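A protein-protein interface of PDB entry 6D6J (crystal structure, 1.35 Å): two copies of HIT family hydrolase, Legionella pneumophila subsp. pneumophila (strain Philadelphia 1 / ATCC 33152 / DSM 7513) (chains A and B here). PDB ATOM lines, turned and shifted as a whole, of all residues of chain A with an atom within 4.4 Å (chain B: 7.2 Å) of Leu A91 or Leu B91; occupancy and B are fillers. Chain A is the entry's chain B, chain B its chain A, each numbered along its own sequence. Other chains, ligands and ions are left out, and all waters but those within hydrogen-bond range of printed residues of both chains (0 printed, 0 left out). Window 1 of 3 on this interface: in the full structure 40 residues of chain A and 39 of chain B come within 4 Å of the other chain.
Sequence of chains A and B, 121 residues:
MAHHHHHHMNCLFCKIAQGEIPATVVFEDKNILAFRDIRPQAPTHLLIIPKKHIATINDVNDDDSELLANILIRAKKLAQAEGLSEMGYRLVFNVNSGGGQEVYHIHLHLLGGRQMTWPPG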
ATOM      1  N   LEU A  72      27.541   4.550 -15.201  1.00  0.00           N
ATOM      2  CA  LEU A  72      26.181   4.143 -15.539  1.00  0.00           C
ATOM      3  C   LEU A  72      25.421   5.271 -16.233  1.00  0.00           C
ATOM      4  O   LEU A  72      24.764   5.048 -17.261  1.00  0.00           O
ATOM      5  CB  LEU A  72      25.479   3.689 -14.261  1.00  0.00           C
ATOM      6  CG  LEU A  72      23.996   3.381 -14.352  1.00  0.00           C
ATOM      7  CD1 LEU A  72      23.710   2.321 -15.389  1.00  0.00           C
ATOM      8  CD2 LEU A  72      23.484   2.925 -12.991  1.00  0.00           C
ATOM      9  N   ALA A  75      26.686   5.567 -19.691  1.00  0.00           N
ATOM     10  CA  ALA A  75      26.160   4.503 -20.547  1.00  0.00           C
ATOM     11  C   ALA A  75      24.759   4.815 -21.066  1.00  0.00           C
ATOM     12  O   ALA A  75      24.461   4.552 -22.238  1.00  0.00           O
ATOM     13  CB  ALA A  75      26.161   3.170 -19.818  1.00  0.00           C
ATOM     14  N   TYR A  89      17.825  -1.822 -24.522  1.00  0.00           N
ATOM     15  CA  TYR A  89      19.198  -2.314 -24.434  1.00  0.00           C
ATOM     16  C   TYR A  89      19.421  -2.876 -23.038  1.00  0.00           C
ATOM     17  O   TYR A  89      18.574  -2.730 -22.148  1.00  0.00           O
ATOM     18  CB  TYR A  89      20.213  -1.213 -24.771  1.00  0.00           C
ATOM     19  CG  TYR A  89      20.134  -0.024 -23.842  1.00  0.00           C
ATOM     20  CD1 TYR A  89      19.296   1.060 -24.121  1.00  0.00           C
ATOM     21  CD2 TYR A  89      20.873   0.009 -22.664  1.00  0.00           C
ATOM     22  CE1 TYR A  89      19.219   2.155 -23.252  1.00  0.00           C
ATOM     23  CE2 TYR A  89      20.813   1.086 -21.813  1.00  0.00           C
ATOM     24  CZ  TYR A  89      20.001   2.153 -22.107  1.00  0.00           C
ATOM     25  OH  TYR A  89      19.967   3.206 -21.228  1.00  0.00           O
ATOM     26  N   ARG A  90      20.572  -3.517 -22.856  1.00  0.00           N
ATOM     27  CA  ARG A  90      20.931  -4.119 -21.583  1.00  0.00           C
ATOM     28  C   ARG A  90      22.279  -3.594 -21.114  1.00  0.00           C
ATOM     29  O   ARG A  90      23.199  -3.376 -21.923  1.00  0.00           O
ATOM     30  CB  ARG A  90      20.974  -5.642 -21.724  1.00  0.00           C
ATOM     31  CG  ARG A  90      21.408  -6.394 -20.452  1.00  0.00           C
ATOM     32  CD  ARG A  90      21.054  -7.869 -20.543  1.00  0.00           C
ATOM     33  NE  ARG A  90      19.602  -8.037 -20.532  1.00  0.00           N
ATOM     34  CZ  ARG A  90      18.943  -9.090 -21.016  1.00  0.00           C
ATOM     35  NH1 ARG A  90      19.599 -10.110 -21.584  1.00  0.00           N
ATOM     36  NH2 ARG A  90      17.614  -9.092 -20.955  1.00  0.00           N
ATOM     37  N   LEU A  91      22.395  -3.393 -19.801  1.00  0.00           N
ATOM     38  CA  LEU A  91      23.634  -2.974 -19.145  1.00  0.00           C
ATOM     39  C   LEU A  91      24.082  -4.084 -18.201  1.00  0.00           C
ATOM     40  O   LEU A  91      23.264  -4.602 -17.426  1.00  0.00           O
ATOM     41  CB  LEU A  91      23.390  -1.692 -18.344  1.00  0.00           C
ATOM     42  CG  LEU A  91      22.974  -0.459 -19.158  1.00  0.00           C
ATOM     43  CD1 LEU A  91      22.578   0.677 -18.245  1.00  0.00           C
ATOM     44  CD2 LEU A  91      24.078  -0.026 -20.096  1.00  0.00           C
ATOM     45  N   VAL A  92      25.362  -4.461 -18.264  1.00  0.00           N
ATOM     46  CA  VAL A  92      25.860  -5.590 -17.472  1.00  0.00           C
ATOM     47  C   VAL A  92      27.199  -5.235 -16.836  1.00  0.00           C
ATOM     48  O   VAL A  92      28.132  -4.829 -17.540  1.00  0.00           O
ATOM     49  CB  VAL A  92      26.048  -6.853 -18.342  1.00  0.00           C
ATOM     50  CG1 VAL A  92      26.506  -8.025 -17.478  1.00  0.00           C
ATOM     51  CG2 VAL A  92      24.762  -7.199 -19.090  1.00  0.00           C
ATOM     52  N   PHE A  93      27.329  -5.474 -15.523  1.00  0.00           N
ATOM     53  CA  PHE A  93      28.641  -5.576 -14.876  1.00  0.00           C
ATOM     54  C   PHE A  93      28.888  -7.039 -14.536  1.00  0.00           C
ATOM     55  O   PHE A  93      28.055  -7.672 -13.878  1.00  0.00           O
ATOM     56  CB  PHE A  93      28.739  -4.810 -13.544  1.00  0.00           C
ATOM     57  CG  PHE A  93      28.831  -3.304 -13.652  1.00  0.00           C
ATOM     58  CD1 PHE A  93      29.970  -2.681 -14.177  1.00  0.00           C
ATOM     59  CD2 PHE A  93      27.808  -2.513 -13.136  1.00  0.00           C
ATOM     60  CE1 PHE A  93      30.055  -1.292 -14.204  1.00  0.00           C
ATOM     61  CE2 PHE A  93      27.891  -1.127 -13.174  1.00  0.00           C
ATOM     62  CZ  PHE A  93      29.019  -0.523 -13.689  1.00  0.00           C
ATOM     63  N   LEU A 108      31.487  -1.449 -17.772  1.00  0.00           N
ATOM     64  CA  LEU A 108      30.055  -1.645 -17.955  1.00  0.00           C
ATOM     65  C   LEU A 108      29.800  -2.009 -19.415  1.00  0.00           C
ATOM     66  O   LEU A 108      30.206  -1.271 -20.326  1.00  0.00           O
ATOM     67  CB  LEU A 108      29.313  -0.358 -17.596  1.00  0.00           C
ATOM     68  CG  LEU A 108      27.787  -0.382 -17.698  1.00  0.00           C
ATOM     69  CD1 LEU A 108      27.225  -1.521 -16.861  1.00  0.00           C
ATOM     70  CD2 LEU A 108      27.244   0.944 -17.180  1.00  0.00           C
ATOM     71  N   HIS A 109      29.127  -3.142 -19.640  1.00  0.00           N
ATOM     72  CA  HIS A 109      28.737  -3.536 -20.988  1.00  0.00           C
ATOM     73  C   HIS A 109      27.418  -2.879 -21.355  1.00  0.00           C
ATOM     74  O   HIS A 109      26.470  -2.889 -20.561  1.00  0.00           O
ATOM     75  CB  HIS A 109      28.488  -5.040 -21.065  1.00  0.00           C
ATOM     76  CG  HIS A 109      29.681  -5.885 -20.796  1.00  0.00           C
ATOM     77  ND1 HIS A 109      30.519  -6.330 -21.799  1.00  0.00           N
ATOM     78  CD2 HIS A 109      30.146  -6.416 -19.642  1.00  0.00           C
ATOM     79  CE1 HIS A 109      31.478  -7.063 -21.262  1.00  0.00           C
ATOM     80  NE2 HIS A 109      31.258  -7.151 -19.959  1.00  0.00           N
ATOM     81  N   LEU A 110      27.350  -2.342 -22.572  1.00  0.00           N
ATOM     82  CA  LEU A 110      26.125  -1.789 -23.139  1.00  0.00           C
ATOM     83  C   LEU A 110      25.834  -2.580 -24.408  1.00  0.00           C
ATOM     84  O   LEU A 110      26.610  -2.515 -25.371  1.00  0.00           O
ATOM     85  CB  LEU A 110      26.316  -0.302 -23.435  1.00  0.00           C
ATOM     86  CG  LEU A 110      25.326   0.391 -24.378  1.00  0.00           C
ATOM     87  CD1 LEU A 110      23.882   0.224 -23.958  1.00  0.00           C
ATOM     88  CD2 LEU A 110      25.691   1.862 -24.486  1.00  0.00           C
ATOM     89  N   ILE B  48      17.186  -5.118  -6.719  1.00  0.00           N
ATOM     90  CA  ILE B  48      17.474  -3.944  -5.897  1.00  0.00           C
ATOM     91  C   ILE B  48      16.780  -2.760  -6.543  1.00  0.00           C
ATOM     92  O   ILE B  48      17.066  -2.431  -7.699  1.00  0.00           O
ATOM     93  CB  ILE B  48      18.989  -3.711  -5.760  1.00  0.00           C
ATOM     94  CG1 ILE B  48      19.654  -4.969  -5.189  1.00  0.00           C
ATOM     95  CG2 ILE B  48      19.248  -2.522  -4.868  1.00  0.00           C
ATOM     96  CD1 ILE B  48      20.932  -5.352  -5.834  1.00  0.00           C
ATOM     97  N   ILE B  57      15.816   3.308 -17.032  1.00  0.00           N
ATOM     98  CA  ILE B  57      17.154   3.900 -17.042  1.00  0.00           C
ATOM     99  C   ILE B  57      17.253   5.011 -18.082  1.00  0.00           C
ATOM    100  O   ILE B  57      18.049   5.945 -17.924  1.00  0.00           O
ATOM    101  CB  ILE B  57      18.218   2.791 -17.217  1.00  0.00           C
ATOM    102  CG1 ILE B  57      18.274   1.919 -15.955  1.00  0.00           C
ATOM    103  CG2 ILE B  57      19.593   3.351 -17.580  1.00  0.00           C
ATOM    104  CD1 ILE B  57      18.907   2.578 -14.738  1.00  0.00           C
ATOM    105  N   ILE B  71      22.564   2.359  -4.918  1.00  0.00           N
ATOM    106  CA  ILE B  71      22.075   1.075  -5.432  1.00  0.00           C
ATOM    107  C   ILE B  71      23.240   0.138  -5.744  1.00  0.00           C
ATOM    108  O   ILE B  71      23.228  -1.047  -5.379  1.00  0.00           O
ATOM    109  CB  ILE B  71      21.180   1.289  -6.664  1.00  0.00           C
ATOM    110  CG1 ILE B  71      19.853   1.947  -6.251  1.00  0.00           C
ATOM    111  CG2 ILE B  71      20.963  -0.034  -7.418  1.00  0.00           C
ATOM    112  CD1 ILE B  71      19.037   2.421  -7.404  1.00  0.00           C
ATOM    113  N   LEU B  72      24.262   0.650  -6.427  1.00  0.00           N
ATOM    114  CA  LEU B  72      25.373  -0.195  -6.853  1.00  0.00           C
ATOM    115  C   LEU B  72      26.205  -0.665  -5.666  1.00  0.00           C
ATOM    116  O   LEU B  72      26.590  -1.834  -5.600  1.00  0.00           O
ATOM    117  CB  LEU B  72      26.229   0.564  -7.866  1.00  0.00           C
ATOM    118  CG  LEU B  72      25.529   0.810  -9.213  1.00  0.00           C
ATOM    119  CD1 LEU B  72      26.247   1.870 -10.032  1.00  0.00           C
ATOM    120  CD2 LEU B  72      25.414  -0.494 -10.000  1.00  0.00           C
ATOM    121  N   ILE B  73      26.488   0.227  -4.711  1.00  0.00           N
ATOM    122  CA  ILE B  73      27.209  -0.180  -3.501  1.00  0.00           C
ATOM    123  C   ILE B  73      26.392  -1.179  -2.695  1.00  0.00           C
ATOM    124  O   ILE B  73      26.938  -2.149  -2.153  1.00  0.00           O
ATOM    125  CB  ILE B  73      27.611   1.056  -2.666  1.00  0.00           C
ATOM    126  CG1 ILE B  73      28.708   1.860  -3.383  1.00  0.00           C
ATOM    127  CG2 ILE B  73      28.044   0.661  -1.242  1.00  0.00           C
ATOM    128  CD1 ILE B  73      30.021   1.125  -3.522  1.00  0.00           C
ATOM    129  N   ALA B  75      24.291  -3.329  -3.892  1.00  0.00           N
ATOM    130  CA  ALA B  75      24.425  -4.593  -4.610  1.00  0.00           C
ATOM    131  C   ALA B  75      25.742  -5.277  -4.257  1.00  0.00           C
ATOM    132  O   ALA B  75      25.779  -6.488  -4.016  1.00  0.00           O
ATOM    133  CB  ALA B  75      24.324  -4.339  -6.122  1.00  0.00           C
ATOM    134  N   LYS B  76      26.842  -4.516  -4.246  1.00  0.00           N
ATOM    135  CA  LYS B  76      28.142  -5.059  -3.856  1.00  0.00           C
ATOM    136  C   LYS B  76      28.085  -5.664  -2.453  1.00  0.00           C
ATOM    137  O   LYS B  76      28.576  -6.777  -2.209  1.00  0.00           O
ATOM    138  CB  LYS B  76      29.186  -3.934  -3.919  1.00  0.00           C
ATOM    139  CG  LYS B  76      30.581  -4.380  -3.499  1.00  0.00           C
ATOM    140  CD  LYS B  76      31.519  -3.214  -3.205  1.00  0.00           C
ATOM    141  CE  LYS B  76      31.082  -2.433  -1.968  1.00  0.00           C
ATOM    142  NZ  LYS B  76      32.182  -1.510  -1.518  1.00  0.00           N
ATOM    143  N   ALA B  79      26.000  -8.867  -2.406  1.00  0.00           N
ATOM    144  CA  ALA B  79      26.788  -9.959  -2.968  1.00  0.00           C
ATOM    145  C   ALA B  79      27.754 -10.511  -1.923  1.00  0.00           C
ATOM    146  O   ALA B  79      27.915 -11.732  -1.803  1.00  0.00           O
ATOM    147  CB  ALA B  79      27.556  -9.476  -4.202  1.00  0.00           C
ATOM    148  N   TYR B  89      29.626 -12.780  -9.535  1.00  0.00           N
ATOM    149  CA  TYR B  89      28.223 -12.414  -9.676  1.00  0.00           C
ATOM    150  C   TYR B  89      28.097 -11.455 -10.851  1.00  0.00           C
ATOM    151  O   TYR B  89      29.095 -10.959 -11.396  1.00  0.00           O
ATOM    152  CB  TYR B  89      27.639 -11.815  -8.388  1.00  0.00           C
ATOM    153  CG  TYR B  89      28.346 -10.585  -7.867  1.00  0.00           C
ATOM    154  CD1 TYR B  89      29.505 -10.687  -7.097  1.00  0.00           C
ATOM    155  CD2 TYR B  89      27.844  -9.306  -8.126  1.00  0.00           C
ATOM    156  CE1 TYR B  89      30.138  -9.540  -6.613  1.00  0.00           C
ATOM    157  CE2 TYR B  89      28.466  -8.166  -7.645  1.00  0.00           C
ATOM    158  CZ  TYR B  89      29.615  -8.288  -6.891  1.00  0.00           C
ATOM    159  OH  TYR B  89      30.220  -7.139  -6.421  1.00  0.00           O
ATOM    160  N   ARG B  90      26.854 -11.214 -11.253  1.00  0.00           N
ATOM    161  CA  ARG B  90      26.550 -10.361 -12.393  1.00  0.00           C
ATOM    162  C   ARG B  90      25.455  -9.380 -11.999  1.00  0.00           C
ATOM    163  O   ARG B  90      24.491  -9.760 -11.323  1.00  0.00           O
ATOM    164  CB  ARG B  90      26.091 -11.226 -13.587  1.00  0.00           C
ATOM    165  CG  ARG B  90      25.644 -10.415 -14.788  1.00  0.00           C
ATOM    166  CD  ARG B  90      25.491 -11.284 -16.032  1.00  0.00           C
ATOM    167  NE  ARG B  90      26.811 -11.747 -16.445  1.00  0.00           N
ATOM    168  CZ  ARG B  90      27.041 -12.753 -17.286  1.00  0.00           C
ATOM    169  NH1 ARG B  90      26.035 -13.441 -17.858  1.00  0.00           N
ATOM    170  NH2 ARG B  90      28.302 -13.069 -17.567  1.00  0.00           N
ATOM    171  N   LEU B  91      25.621  -8.116 -12.401  1.00  0.00           N
ATOM    172  CA  LEU B  91      24.639  -7.059 -12.187  1.00  0.00           C
ATOM    173  C   LEU B  91      24.052  -6.674 -13.534  1.00  0.00           C
ATOM    174  O   LEU B  91      24.807  -6.446 -14.483  1.00  0.00           O
ATOM    175  CB  LEU B  91      25.313  -5.836 -11.555  1.00  0.00           C
ATOM    176  CG  LEU B  91      26.053  -6.101 -10.248  1.00  0.00           C
ATOM    177  CD1 LEU B  91      26.691  -4.830  -9.726  1.00  0.00           C
ATOM    178  CD2 LEU B  91      25.117  -6.709  -9.195  1.00  0.00           C
ATOM    179  N   VAL B  92      22.714  -6.602 -13.622  1.00  0.00           N
ATOM    180  CA  VAL B  92      22.043  -6.338 -14.899  1.00  0.00           C
ATOM    181  C   VAL B  92      20.960  -5.276 -14.733  1.00  0.00           C
ATOM    182  O   VAL B  92      20.090  -5.407 -13.861  1.00  0.00           O
ATOM    183  CB  VAL B  92      21.410  -7.612 -15.487  1.00  0.00           C
ATOM    184  CG1 VAL B  92      20.759  -7.330 -16.841  1.00  0.00           C
ATOM    185  CG2 VAL B  92      22.419  -8.733 -15.611  1.00  0.00           C
ATOM    186  N   PHE B  93      20.978  -4.256 -15.601  1.00  0.00           N
ATOM    187  CA  PHE B  93      19.803  -3.416 -15.822  1.00  0.00           C
ATOM    188  C   PHE B  93      19.246  -3.730 -17.203  1.00  0.00           C
ATOM    189  O   PHE B  93      19.984  -3.685 -18.201  1.00  0.00           O
ATOM    190  CB  PHE B  93      20.131  -1.917 -15.818  1.00  0.00           C
ATOM    191  CG  PHE B  93      20.232  -1.278 -14.453  1.00  0.00           C
ATOM    192  CD1 PHE B  93      19.106  -1.171 -13.623  1.00  0.00           C
ATOM    193  CD2 PHE B  93      21.422  -0.705 -14.027  1.00  0.00           C
ATOM    194  CE1 PHE B  93      19.191  -0.550 -12.387  1.00  0.00           C
ATOM    195  CE2 PHE B  93      21.495  -0.080 -12.780  1.00  0.00           C
ATOM    196  CZ  PHE B  93      20.377   0.000 -11.985  1.00  0.00           C
ATOM    197  N   ASN B  94      17.955  -4.018 -17.267  1.00  0.00           N
ATOM    198  CA  ASN B  94      17.230  -4.096 -18.532  1.00  0.00           C
ATOM    199  C   ASN B  94      16.584  -2.747 -18.796  1.00  0.00           C
ATOM    200  O   ASN B  94      15.969  -2.173 -17.896  1.00  0.00           O
ATOM    201  CB  ASN B  94      16.151  -5.181 -18.464  1.00  0.00           C
ATOM    202  CG  ASN B  94      16.735  -6.567 -18.406  1.00  0.00           C
ATOM    203  OD1 ASN B  94      17.922  -6.769 -18.654  1.00  0.00           O
ATOM    204  ND2 ASN B  94      15.895  -7.540 -18.108  1.00  0.00           N
ATOM    205  N   VAL B  95      16.700  -2.252 -20.027  1.00  0.00           N
ATOM    206  CA  VAL B  95      16.212  -0.913 -20.353  1.00  0.00           C
ATOM    207  C   VAL B  95      15.237  -1.000 -21.521  1.00  0.00           C
ATOM    208  O   VAL B  95      15.641  -1.279 -22.663  1.00  0.00           O
ATOM    209  CB  VAL B  95      17.344   0.084 -20.620  1.00  0.00           C
ATOM    210  CG1 VAL B  95      16.750   1.498 -20.762  1.00  0.00           C
ATOM    211  CG2 VAL B  95      18.417   0.009 -19.518  1.00  0.00           C
ATOM    212  N   GLY B  99      15.372  -4.364 -24.197  1.00  0.00           N
ATOM    213  CA  GLY B  99      16.299  -4.782 -23.174  1.00  0.00           C
ATOM    214  C   GLY B  99      15.754  -5.832 -22.244  1.00  0.00           C
ATOM    215  O   GLY B  99      16.499  -6.347 -21.412  1.00  0.00           O
ATOM    216  N   LEU B 108      17.730  -3.244 -10.383  1.00  0.00           N
ATOM    217  CA  LEU B 108      19.004  -3.885 -10.674  1.00  0.00           C
ATOM    218  C   LEU B 108      18.904  -5.358 -10.300  1.00  0.00           C
ATOM    219  O   LEU B 108      18.534  -5.690  -9.165  1.00  0.00           O
ATOM    220  CB  LEU B 108      20.108  -3.219  -9.852  1.00  0.00           C
ATOM    221  CG  LEU B 108      21.520  -3.755 -10.096  1.00  0.00           C
ATOM    222  CD1 LEU B 108      21.932  -3.525 -11.551  1.00  0.00           C
ATOM    223  CD2 LEU B 108      22.516  -3.094  -9.161  1.00  0.00           C
ATOM    224  N   HIS B 109      19.224  -6.241 -11.243  1.00  0.00           N
ATOM    225  CA  HIS B 109      19.301  -7.670 -10.954  1.00  0.00           C
ATOM    226  C   HIS B 109      20.697  -8.002 -10.448  1.00  0.00           C
ATOM    227  O   HIS B 109      21.693  -7.572 -11.035  1.00  0.00           O
ATOM    228  CB  HIS B 109      19.111  -8.504 -12.225  1.00  0.00           C
ATOM    229  CG  HIS B 109      17.778  -8.350 -12.873  1.00  0.00           C
ATOM    230  ND1 HIS B 109      16.735  -9.232 -12.654  1.00  0.00           N
ATOM    231  CD2 HIS B 109      17.328  -7.426 -13.752  1.00  0.00           C
ATOM    232  CE1 HIS B 109      15.691  -8.837 -13.365  1.00  0.00           C
ATOM    233  NE2 HIS B 109      16.026  -7.750 -14.045  1.00  0.00           N
ATOM    234  N   LEU B 110      20.760  -8.796  -9.382  1.00  0.00           N
ATOM    235  CA  LEU B 110      22.007  -9.358  -8.870  1.00  0.00           C
ATOM    236  C   LEU B 110      21.881 -10.872  -8.976  1.00  0.00           C
ATOM    237  O   LEU B 110      21.001 -11.473  -8.341  1.00  0.00           O
ATOM    238  CB  LEU B 110      22.255  -8.913  -7.422  1.00  0.00           C
ATOM    239  CG  LEU B 110      23.254  -9.727  -6.568  1.00  0.00           C
ATOM    240  CD1 LEU B 110      24.644  -9.763  -7.175  1.00  0.00           C
ATOM    241  CD2 LEU B 110      23.329  -9.212  -5.128  1.00  0.00           C
ATOM    242  N   LEU B 111      22.744 -11.482  -9.781  1.00  0.00           N
ATOM    243  CA  LEU B 111      22.680 -12.915 -10.057  1.00  0.00           C
ATOM    244  C   LEU B 111      23.997 -13.581  -9.706  1.00  0.00           C
ATOM    245  O   LEU B 111      25.061 -13.061 -10.031  1.00  0.00           O
ATOM    246  CB  LEU B 111      22.408 -13.148 -11.548  1.00  0.00           C
ATOM    247  CG  LEU B 111      21.062 -12.623 -12.033  1.00  0.00           C
ATOM    248  CD1 LEU B 111      21.237 -11.878 -13.337  1.00  0.00           C
ATOM    249  CD2 LEU B 111      20.134 -13.800 -12.173  1.00  0.00           C
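O of Phe B93 is in hydrogen-bond range of N of Leu A91 (2.9 Å). The backbone carbonyl oxygen of Phe A93 lies within hydrogen-bond range of the backbone NH of Leu B91 (2.9 Å). The side-chain amide oxygen of Asn B94 is in hydrogen-bond range of the guanidinium group of Arg A90 (2.8 Å). The backbone NH of Val B95 sits at hydrogen-bond distance from the backbone carbonyl oxygen of Tyr A89, at 2.9 Å. The backbone carbonyl oxygen (O) of Gly B99 is in hydrogen-bond range of the guanidinium group (NH2) of Arg A90 (3.0 Å).
The backbone carbonyl oxygen (O) of Val A92 is in hydrogen-bond range of the backbone NH (N) of His A109, 2.9 Å away. The backbone NH of Arg B90 sits at hydrogen-bond distance from the backbone carbonyl oxygen of Leu B111 (2.8 Å). O of Val B92 lies within hydrogen-bond range of N of His B109, at 2.9 Å. O of Gly B99 sits close to OD1 of Asn B94 (3.1 Å).
Leu A72 touches Phe B93 (CD2 to CE2, 3.6 Å). Tyr A89 touches Ile B57 (OH to CG2, 3.7 Å). Tyr A89 touches Asn B94 (O to C, 3.9 Å). Tyr A89 touches Gly B99. Arg A90 touches Val B92 (CD to CG1, 3.8 Å). Leu A91 touches Leu B91. Val B92 touches Leu A91 (CA to O, 3.3 Å). CG of Arg B90 touches CG1 of Val A92, 3.7 Å away. O of Leu B91 touches CA of Val A92, at 3.3 Å. Phe A93 touches Arg B90.
Of the printed residues of chain B, Leu A72 touches Phe B93 (3.6 Å). Printed residues of chain B within 4 Å of Leu A91: Leu B91, Val B92 and Phe B93. Leu A110 touches none of the printed residues of chain B. Ala B75 touches none of the printed residues of chain A. Of chain A, only Leu A91 (3.8 Å), Val A92 (3.3 Å) and Phe A93 (2.9 Å) come within 4 Å of Leu B91. Of the printed residues of chain A, Val B92 touches Arg A90 and Leu A91. Of the printed residues of chain A, Phe B93 touches Leu A72, Arg A90 and Leu A91. Of the printed residues of chain A, Asn B94 touches Tyr A89 (3.9 Å) and Arg A90 (2.8 Å). Printed residues of chain A within 4 Å of Gly B99: Tyr A89 (3.2 Å) and Arg A90 (3.0 Å). The nearest printed residue of chain A that does not touch Leu B91 is Leu A108 (6.0 Å). The nearest printed residue of chain A that does not touch Ile B57 is Leu A91 (4.1 Å).
Printed residues of chain A that touch a printed residue of chain B: Leu A72, Tyr A89, Arg A90, Leu A91, Val A92 and Phe A93. Hydrophobic or aromatic side chains of chain A that line the printed part of chain B: Leu A72, Tyr A89, Leu A91 and Val A92. Of the 20 printed residues of chain B, 8 touch a printed residue of chain A. Printed residues of chain B that touch a printed residue of chain A: Ile B57, Arg B90, Leu B91, Val B92, Phe B93, Asn B94, Val B95 and Gly B99. Hydrophobic or aromatic side chains of chain B within 4 Å of the printed part of chain A: Ile B57, Val B92, Phe B93 and Val B95.
Leu A72 touches Phe B93, but with the chains exchanged Phe A93 does not touch Leu B72 (4.1 Å). Arg A90 touches Val B92, and with the chains exchanged Val A92 touches Arg B90. Leu A91 touches its own counterpart, Leu B91. Leu A91 touches Phe B93, and with the chains exchanged Phe A93 touches Leu B91. Positions printed for both chains: 72, 75, 89, 90, 91, 92, 93, 108, 109 and 110.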
